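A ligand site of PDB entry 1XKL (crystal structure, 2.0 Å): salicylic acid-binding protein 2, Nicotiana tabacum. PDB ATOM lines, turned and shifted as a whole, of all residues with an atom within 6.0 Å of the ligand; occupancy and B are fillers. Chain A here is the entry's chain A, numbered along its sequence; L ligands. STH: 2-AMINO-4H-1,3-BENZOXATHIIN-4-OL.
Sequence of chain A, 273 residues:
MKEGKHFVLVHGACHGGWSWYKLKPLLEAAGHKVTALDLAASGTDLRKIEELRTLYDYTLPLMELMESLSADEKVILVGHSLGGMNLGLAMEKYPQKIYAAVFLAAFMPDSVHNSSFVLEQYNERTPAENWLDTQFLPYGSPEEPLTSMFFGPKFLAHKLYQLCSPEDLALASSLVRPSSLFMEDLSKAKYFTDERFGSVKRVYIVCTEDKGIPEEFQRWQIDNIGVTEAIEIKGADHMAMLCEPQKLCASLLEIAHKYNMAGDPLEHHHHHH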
ATOM      1  N   HIS A  11     -21.637  21.256  21.247  1.00  0.00           N
ATOM      2  CA  HIS A  11     -20.932  20.169  21.913  1.00  0.00           C
ATOM      3  C   HIS A  11     -20.416  19.087  20.965  1.00  0.00           C
ATOM      4  O   HIS A  11     -20.767  19.056  19.787  1.00  0.00           O
ATOM      5  CB  HIS A  11     -21.872  19.532  22.945  1.00  0.00           C
ATOM      6  CG  HIS A  11     -23.049  18.853  22.335  1.00  0.00           C
ATOM      7  ND1 HIS A  11     -22.978  17.606  21.749  1.00  0.00           N
ATOM      8  CD2 HIS A  11     -24.326  19.264  22.185  1.00  0.00           C
ATOM      9  CE1 HIS A  11     -24.165  17.278  21.263  1.00  0.00           C
ATOM     10  NE2 HIS A  11     -24.997  18.265  21.514  1.00  0.00           N
ATOM     11  N   GLY A  12     -19.601  18.200  21.511  1.00  0.00           N
ATOM     12  CA  GLY A  12     -19.025  17.109  20.745  1.00  0.00           C
ATOM     13  C   GLY A  12     -19.840  15.831  20.884  1.00  0.00           C
ATOM     14  O   GLY A  12     -20.936  15.847  21.459  1.00  0.00           O
ATOM     15  N   ALA A  13     -19.308  14.729  20.388  1.00  0.00           N
ATOM     16  CA  ALA A  13     -19.993  13.450  20.435  1.00  0.00           C
ATOM     17  C   ALA A  13     -20.184  12.891  21.837  1.00  0.00           C
ATOM     18  O   ALA A  13     -19.299  12.974  22.688  1.00  0.00           O
ATOM     19  CB  ALA A  13     -19.250  12.433  19.573  1.00  0.00           C
ATOM     20  N   CYS A  14     -21.351  12.300  22.053  1.00  0.00           N
ATOM     21  CA  CYS A  14     -21.704  11.703  23.336  1.00  0.00           C
ATOM     22  C   CYS A  14     -21.938  12.742  24.426  1.00  0.00           C
ATOM     23  O   CYS A  14     -22.221  12.375  25.570  1.00  0.00           O
ATOM     24  CB  CYS A  14     -20.604  10.729  23.792  1.00  0.00           C
ATOM     25  SG  CYS A  14     -20.280   9.328  22.668  1.00  0.00           S
ATOM     26  N   HIS A  15     -21.838  14.026  24.086  1.00  0.00           N
ATOM     27  CA  HIS A  15     -22.059  15.082  25.072  1.00  0.00           C
ATOM     28  C   HIS A  15     -23.314  15.902  24.763  1.00  0.00           C
ATOM     29  O   HIS A  15     -24.133  15.492  23.942  1.00  0.00           O
ATOM     30  CB  HIS A  15     -20.828  16.006  25.162  1.00  0.00           C
ATOM     31  CG  HIS A  15     -19.663  15.363  25.830  1.00  0.00           C
ATOM     32  ND1 HIS A  15     -19.012  14.267  25.300  1.00  0.00           N
ATOM     33  CD2 HIS A  15     -19.051  15.626  27.013  1.00  0.00           C
ATOM     34  CE1 HIS A  15     -18.057  13.877  26.123  1.00  0.00           C
ATOM     35  NE2 HIS A  15     -18.052  14.689  27.173  1.00  0.00           N
ATOM     36  N   HIS A  80     -17.000  22.108  19.546  1.00  0.00           N
ATOM     37  CA  HIS A  80     -16.060  21.297  20.303  1.00  0.00           C
ATOM     38  C   HIS A  80     -16.057  19.855  19.805  1.00  0.00           C
ATOM     39  O   HIS A  80     -17.109  19.285  19.521  1.00  0.00           O
ATOM     40  CB  HIS A  80     -16.448  21.339  21.784  1.00  0.00           C
ATOM     41  CG  HIS A  80     -15.676  20.372  22.636  1.00  0.00           C
ATOM     42  ND1 HIS A  80     -16.258  19.273  23.230  1.00  0.00           N
ATOM     43  CD2 HIS A  80     -14.363  20.339  22.983  1.00  0.00           C
ATOM     44  CE1 HIS A  80     -15.341  18.605  23.904  1.00  0.00           C
ATOM     45  NE2 HIS A  80     -14.194  19.225  23.772  1.00  0.00           N
ATOM     46  N   SER A  81     -14.861  19.281  19.687  1.00  0.00           N
ATOM     47  CA  SER A  81     -14.704  18.012  19.269  1.00  0.00           C
ATOM     48  C   SER A  81     -15.449  17.734  17.944  1.00  0.00           C
ATOM     49  O   SER A  81     -15.212  18.443  16.963  1.00  0.00           O
ATOM     50  CB  SER A  81     -15.181  17.095  20.396  1.00  0.00           C
ATOM     51  OG  SER A  81     -14.792  15.785  20.658  1.00  0.00           O
ATOM     52  N   LEU A  82     -16.351  16.745  17.908  1.00  0.00           N
ATOM     53  CA  LEU A  82     -17.126  16.407  16.714  1.00  0.00           C
ATOM     54  C   LEU A  82     -18.018  17.562  16.314  1.00  0.00           C
ATOM     55  O   LEU A  82     -18.546  17.603  15.202  1.00  0.00           O
ATOM     56  CB  LEU A  82     -17.992  15.159  16.963  1.00  0.00           C
ATOM     57  CG  LEU A  82     -18.898  14.677  15.811  1.00  0.00           C
ATOM     58  CD1 LEU A  82     -18.015  14.325  14.616  1.00  0.00           C
ATOM     59  CD2 LEU A  82     -19.726  13.450  16.226  1.00  0.00           C
ATOM     60  N   GLY A  83     -18.188  18.518  17.227  1.00  0.00           N
ATOM     61  CA  GLY A  83     -19.034  19.670  16.968  1.00  0.00           C
ATOM     62  C   GLY A  83     -18.544  20.504  15.797  1.00  0.00           C
ATOM     63  O   GLY A  83     -19.321  21.219  15.164  1.00  0.00           O
ATOM     64  N   PHE A 107     -12.861  18.704  15.109  1.00  0.00           N
ATOM     65  CA  PHE A 107     -12.569  18.134  13.816  1.00  0.00           C
ATOM     66  C   PHE A 107     -12.994  19.262  12.890  1.00  0.00           C
ATOM     67  O   PHE A 107     -14.156  19.671  12.899  1.00  0.00           O
ATOM     68  CB  PHE A 107     -13.409  16.887  13.534  1.00  0.00           C
ATOM     69  CG  PHE A 107     -12.948  15.671  14.273  1.00  0.00           C
ATOM     70  CD1 PHE A 107     -13.818  14.986  15.120  1.00  0.00           C
ATOM     71  CD2 PHE A 107     -11.643  15.196  14.110  1.00  0.00           C
ATOM     72  CE1 PHE A 107     -13.396  13.846  15.799  1.00  0.00           C
ATOM     73  CE2 PHE A 107     -11.208  14.062  14.784  1.00  0.00           C
ATOM     74  CZ  PHE A 107     -12.085  13.379  15.638  1.00  0.00           C
ATOM     75  N   LEU A 119     -11.938  12.827   9.634  1.00  0.00           N
ATOM     76  CA  LEU A 119     -12.279  11.706  10.493  1.00  0.00           C
ATOM     77  C   LEU A 119     -11.443  10.496  10.098  1.00  0.00           C
ATOM     78  O   LEU A 119     -10.966   9.750  10.957  1.00  0.00           O
ATOM     79  CB  LEU A 119     -13.775  11.387  10.391  1.00  0.00           C
ATOM     80  CG  LEU A 119     -14.705  12.490  10.931  1.00  0.00           C
ATOM     81  CD1 LEU A 119     -16.148  12.008  10.917  1.00  0.00           C
ATOM     82  CD2 LEU A 119     -14.290  12.847  12.349  1.00  0.00           C
ATOM     83  N   TYR A 122      -7.829  11.216  11.250  1.00  0.00           N
ATOM     84  CA  TYR A 122      -7.763  11.025  12.705  1.00  0.00           C
ATOM     85  C   TYR A 122      -7.580   9.540  13.034  1.00  0.00           C
ATOM     86  O   TYR A 122      -6.678   9.177  13.787  1.00  0.00           O
ATOM     87  CB  TYR A 122      -9.051  11.531  13.359  1.00  0.00           C
ATOM     88  CG  TYR A 122      -9.150  11.153  14.824  1.00  0.00           C
ATOM     89  CD1 TYR A 122      -8.401  11.828  15.785  1.00  0.00           C
ATOM     90  CD2 TYR A 122      -9.939  10.083  15.236  1.00  0.00           C
ATOM     91  CE1 TYR A 122      -8.431  11.436  17.123  1.00  0.00           C
ATOM     92  CE2 TYR A 122      -9.974   9.672  16.562  1.00  0.00           C
ATOM     93  CZ  TYR A 122      -9.211  10.356  17.504  1.00  0.00           C
ATOM     94  OH  TYR A 122      -9.216   9.941  18.817  1.00  0.00           O
ATOM     95  N   TRP A 131      -8.994   3.912  22.188  1.00  0.00           N
ATOM     96  CA  TRP A 131     -10.438   3.929  22.464  1.00  0.00           C
ATOM     97  C   TRP A 131     -10.840   3.303  23.796  1.00  0.00           C
ATOM     98  O   TRP A 131     -11.951   3.544  24.282  1.00  0.00           O
ATOM     99  CB  TRP A 131     -11.201   3.231  21.332  1.00  0.00           C
ATOM    100  CG  TRP A 131     -11.150   3.975  20.034  1.00  0.00           C
ATOM    101  CD1 TRP A 131     -10.413   3.636  18.925  1.00  0.00           C
ATOM    102  CD2 TRP A 131     -11.809   5.203  19.723  1.00  0.00           C
ATOM    103  NE1 TRP A 131     -10.587   4.582  17.938  1.00  0.00           N
ATOM    104  CE2 TRP A 131     -11.435   5.554  18.402  1.00  0.00           C
ATOM    105  CE3 TRP A 131     -12.693   6.046  20.419  1.00  0.00           C
ATOM    106  CZ2 TRP A 131     -11.908   6.703  17.771  1.00  0.00           C
ATOM    107  CZ3 TRP A 131     -13.154   7.187  19.788  1.00  0.00           C
ATOM    108  CH2 TRP A 131     -12.756   7.511  18.471  1.00  0.00           C
ATOM    109  N   MET A 149     -21.203   5.205  18.355  1.00  0.00           N
ATOM    110  CA  MET A 149     -20.024   5.332  19.206  1.00  0.00           C
ATOM    111  C   MET A 149     -20.463   5.753  20.597  1.00  0.00           C
ATOM    112  O   MET A 149     -21.211   6.723  20.750  1.00  0.00           O
ATOM    113  CB  MET A 149     -19.063   6.371  18.613  1.00  0.00           C
ATOM    114  CG  MET A 149     -17.806   6.613  19.427  1.00  0.00           C
ATOM    115  SD  MET A 149     -16.617   7.915  18.591  1.00  0.00           S
ATOM    116  CE  MET A 149     -17.802   9.447  18.661  1.00  0.00           C
ATOM    117  N   PHE A 151     -18.725   6.464  24.334  1.00  0.00           N
ATOM    118  CA  PHE A 151     -17.571   6.537  25.223  1.00  0.00           C
ATOM    119  C   PHE A 151     -17.810   5.747  26.506  1.00  0.00           C
ATOM    120  O   PHE A 151     -18.899   5.764  27.060  1.00  0.00           O
ATOM    121  CB  PHE A 151     -17.269   7.998  25.588  1.00  0.00           C
ATOM    122  CG  PHE A 151     -16.931   8.870  24.407  1.00  0.00           C
ATOM    123  CD1 PHE A 151     -16.361   8.320  23.260  1.00  0.00           C
ATOM    124  CD2 PHE A 151     -17.155  10.246  24.451  1.00  0.00           C
ATOM    125  CE1 PHE A 151     -16.016   9.129  22.176  1.00  0.00           C
ATOM    126  CE2 PHE A 151     -16.806  11.064  23.368  1.00  0.00           C
ATOM    127  CZ  PHE A 151     -16.235  10.500  22.226  1.00  0.00           C
ATOM    128  N   PHE A 155     -12.354   5.478  29.051  1.00  0.00           N
ATOM    129  CA  PHE A 155     -12.009   6.394  27.973  1.00  0.00           C
ATOM    130  C   PHE A 155     -12.186   7.831  28.400  1.00  0.00           C
ATOM    131  O   PHE A 155     -11.361   8.697  28.089  1.00  0.00           O
ATOM    132  CB  PHE A 155     -12.859   6.114  26.734  1.00  0.00           C
ATOM    133  CG  PHE A 155     -12.539   6.986  25.551  1.00  0.00           C
ATOM    134  CD1 PHE A 155     -13.356   8.057  25.206  1.00  0.00           C
ATOM    135  CD2 PHE A 155     -11.398   6.735  24.777  1.00  0.00           C
ATOM    136  CE1 PHE A 155     -13.061   8.855  24.095  1.00  0.00           C
ATOM    137  CE2 PHE A 155     -11.098   7.529  23.672  1.00  0.00           C
ATOM    138  CZ  PHE A 155     -11.926   8.593  23.332  1.00  0.00           C
ATOM    139  N   LEU A 160     -10.097  11.789  28.010  1.00  0.00           N
ATOM    140  CA  LEU A 160     -10.798  13.045  27.845  1.00  0.00           C
ATOM    141  C   LEU A 160     -10.765  13.982  29.058  1.00  0.00           C
ATOM    142  O   LEU A 160     -10.612  15.190  28.902  1.00  0.00           O
ATOM    143  CB  LEU A 160     -12.255  12.772  27.444  1.00  0.00           C
ATOM    144  CG  LEU A 160     -12.549  11.995  26.150  1.00  0.00           C
ATOM    145  CD1 LEU A 160     -14.017  12.171  25.769  1.00  0.00           C
ATOM    146  CD2 LEU A 160     -11.665  12.482  25.036  1.00  0.00           C
ATOM    147  N   SER A 180     -22.302   9.063  17.084  1.00  0.00           N
ATOM    148  CA  SER A 180     -21.758   8.436  15.870  1.00  0.00           C
ATOM    149  C   SER A 180     -20.818   9.420  15.208  1.00  0.00           C
ATOM    150  O   SER A 180     -20.927  10.620  15.429  1.00  0.00           O
ATOM    151  CB  SER A 180     -22.925   8.079  14.940  1.00  0.00           C
ATOM    152  OG  SER A 180     -22.499   7.532  13.705  1.00  0.00           O
ATOM    153  N   LEU A 181     -19.878   8.916  14.407  1.00  0.00           N
ATOM    154  CA  LEU A 181     -18.963   9.797  13.687  1.00  0.00           C
ATOM    155  C   LEU A 181     -19.563   9.982  12.309  1.00  0.00           C
ATOM    156  O   LEU A 181     -19.079  10.792  11.516  1.00  0.00           O
ATOM    157  CB  LEU A 181     -17.578   9.165  13.565  1.00  0.00           C
ATOM    158  CG  LEU A 181     -16.763   9.010  14.849  1.00  0.00           C
ATOM    159  CD1 LEU A 181     -15.411   8.378  14.558  1.00  0.00           C
ATOM    160  CD2 LEU A 181     -16.572  10.379  15.491  1.00  0.00           C
ATOM    161  N   GLY A 212      -7.606  12.890  23.699  1.00  0.00           N
ATOM    162  CA  GLY A 212      -8.629  12.259  22.879  1.00  0.00           C
ATOM    163  C   GLY A 212      -8.303  12.493  21.417  1.00  0.00           C
ATOM    164  O   GLY A 212      -8.224  11.571  20.605  1.00  0.00           O
ATOM    165  N   ILE A 213      -8.113  13.771  21.118  1.00  0.00           N
ATOM    166  CA  ILE A 213      -7.729  14.246  19.807  1.00  0.00           C
ATOM    167  C   ILE A 213      -6.422  14.951  20.164  1.00  0.00           C
ATOM    168  O   ILE A 213      -6.404  16.147  20.472  1.00  0.00           O
ATOM    169  CB  ILE A 213      -8.735  15.269  19.252  1.00  0.00           C
ATOM    170  CG1 ILE A 213     -10.124  14.639  19.156  1.00  0.00           C
ATOM    171  CG2 ILE A 213      -8.267  15.761  17.899  1.00  0.00           C
ATOM    172  CD1 ILE A 213     -11.146  15.516  18.441  1.00  0.00           C
ATOM    173  N   HIS A 238      -8.817  17.529  26.696  1.00  0.00           N
ATOM    174  CA  HIS A 238      -9.866  17.634  25.689  1.00  0.00           C
ATOM    175  C   HIS A 238     -11.070  18.480  26.111  1.00  0.00           C
ATOM    176  O   HIS A 238     -11.716  19.100  25.266  1.00  0.00           O
ATOM    177  CB  HIS A 238     -10.361  16.242  25.295  1.00  0.00           C
ATOM    178  CG  HIS A 238     -11.257  16.233  24.104  1.00  0.00           C
ATOM    179  ND1 HIS A 238     -10.835  16.657  22.858  1.00  0.00           N
ATOM    180  CD2 HIS A 238     -12.564  15.925  23.960  1.00  0.00           C
ATOM    181  CE1 HIS A 238     -11.843  16.602  22.011  1.00  0.00           C
ATOM    182  NE2 HIS A 238     -12.906  16.158  22.659  1.00  0.00           N
ATOM    183  N   MET A 239     -11.361  18.504  27.408  1.00  0.00           N
ATOM    184  CA  MET A 239     -12.509  19.245  27.915  1.00  0.00           C
ATOM    185  C   MET A 239     -12.119  20.618  28.470  1.00  0.00           C
ATOM    186  O   MET A 239     -12.326  20.905  29.657  1.00  0.00           O
ATOM    187  CB  MET A 239     -13.219  18.438  29.002  1.00  0.00           C
ATOM    188  CG  MET A 239     -14.567  17.846  28.584  1.00  0.00           C
ATOM    189  SD  MET A 239     -14.493  16.748  26.995  1.00  0.00           S
ATOM    190  CE  MET A 239     -12.973  15.684  27.471  1.00  0.00           C
HETATM  191  C8  STH L   1     -15.601  13.086  19.019  1.00  0.00           C
HETATM  192  O8  STH L   1     -16.097  12.759  17.796  1.00  0.00           O
HETATM  193  C1  STH L   1     -14.329  12.506  19.540  1.00  0.00           C
HETATM  194  C2  STH L   1     -13.840  12.893  20.890  1.00  0.00           C
HETATM  195  C3  STH L   1     -12.629  12.324  21.380  1.00  0.00           C
HETATM  196  C4  STH L   1     -11.896  11.379  20.596  1.00  0.00           C
HETATM  197  C5  STH L   1     -12.371  10.996  19.298  1.00  0.00           C
HETATM  198  C6  STH L   1     -13.568  11.537  18.789  1.00  0.00           C
HETATM  199  C7  STH L   1     -15.526  14.643  21.074  1.00  0.00           C
HETATM  200  O2  STH L   1     -14.528  13.829  21.690  1.00  0.00           O
HETATM  201  N7  STH L   1     -16.429  15.020  22.062  1.00  0.00           N
HETATM  202  S7  STH L   1     -16.305  14.024  19.804  1.00  0.00           S
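An oxygen (O2) of the ligand is in hydrogen-bond range of a ring nitrogen (NE2) of His 238 (3.0 Å). N of Leu 82 lies close to S7 of the ligand (3.3 Å). The side-chain hydroxyl (OG) of Ser 81 is bonded to a carbon (C7) of the ligand (1.4 Å). N of Ala 13 sits close to S7 of the ligand, at 3.1 Å.
The backbone NH of Gly 12 lies close to the backbone carbonyl oxygen of His 80 (3.4 Å). The side-chain hydroxyl of Tyr 122 lies within hydrogen-bond range of the backbone carbonyl oxygen of Gly 212 (2.6 Å). The backbone carbonyl oxygen of Ser 81 is in hydrogen-bond range of the backbone NH of Phe 107. The backbone carbonyl oxygen (O) of Phe 155 lies within hydrogen-bond range of the backbone NH (N) of Leu 160, at 3.3 Å. SG of Cys 14 lies within hydrogen-bond range of N of Phe 151. A ring nitrogen (NE2) of His 238 lies within hydrogen-bond range of the side-chain hydroxyl of Ser 81. NE2 of His 80 sits at hydrogen-bond distance from O of His 238 (2.9 Å). O of Ala 13 sits at hydrogen-bond distance from ND1 of His 15, at 2.9 Å.
Residues that only touch the ligand: Leu 181, Tyr 122, Phe 107, Gly 12, Trp 131, Phe 151, Gly 212, Leu 160, Met 149, Phe 155 and Ile 213. Hydrophobic or aromatic side chains that line the ligand: Ala 13, Leu 82, Phe 107, Tyr 122, Trp 131, Met 149, Phe 151, Phe 155, Leu 160, Leu 181, Ile 213 and His 238. Within 4 Å of the ligand: Gly 12, Ala 13, Ser 81, Leu 82, Phe 107, Tyr 122, Trp 131, Met 149, Phe 151, Phe 155, Leu 160, Leu 181, Gly 212, Ile 213 and His 238. The nearest printed residue that does not touch the ligand is His 80 (4.2 Å).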
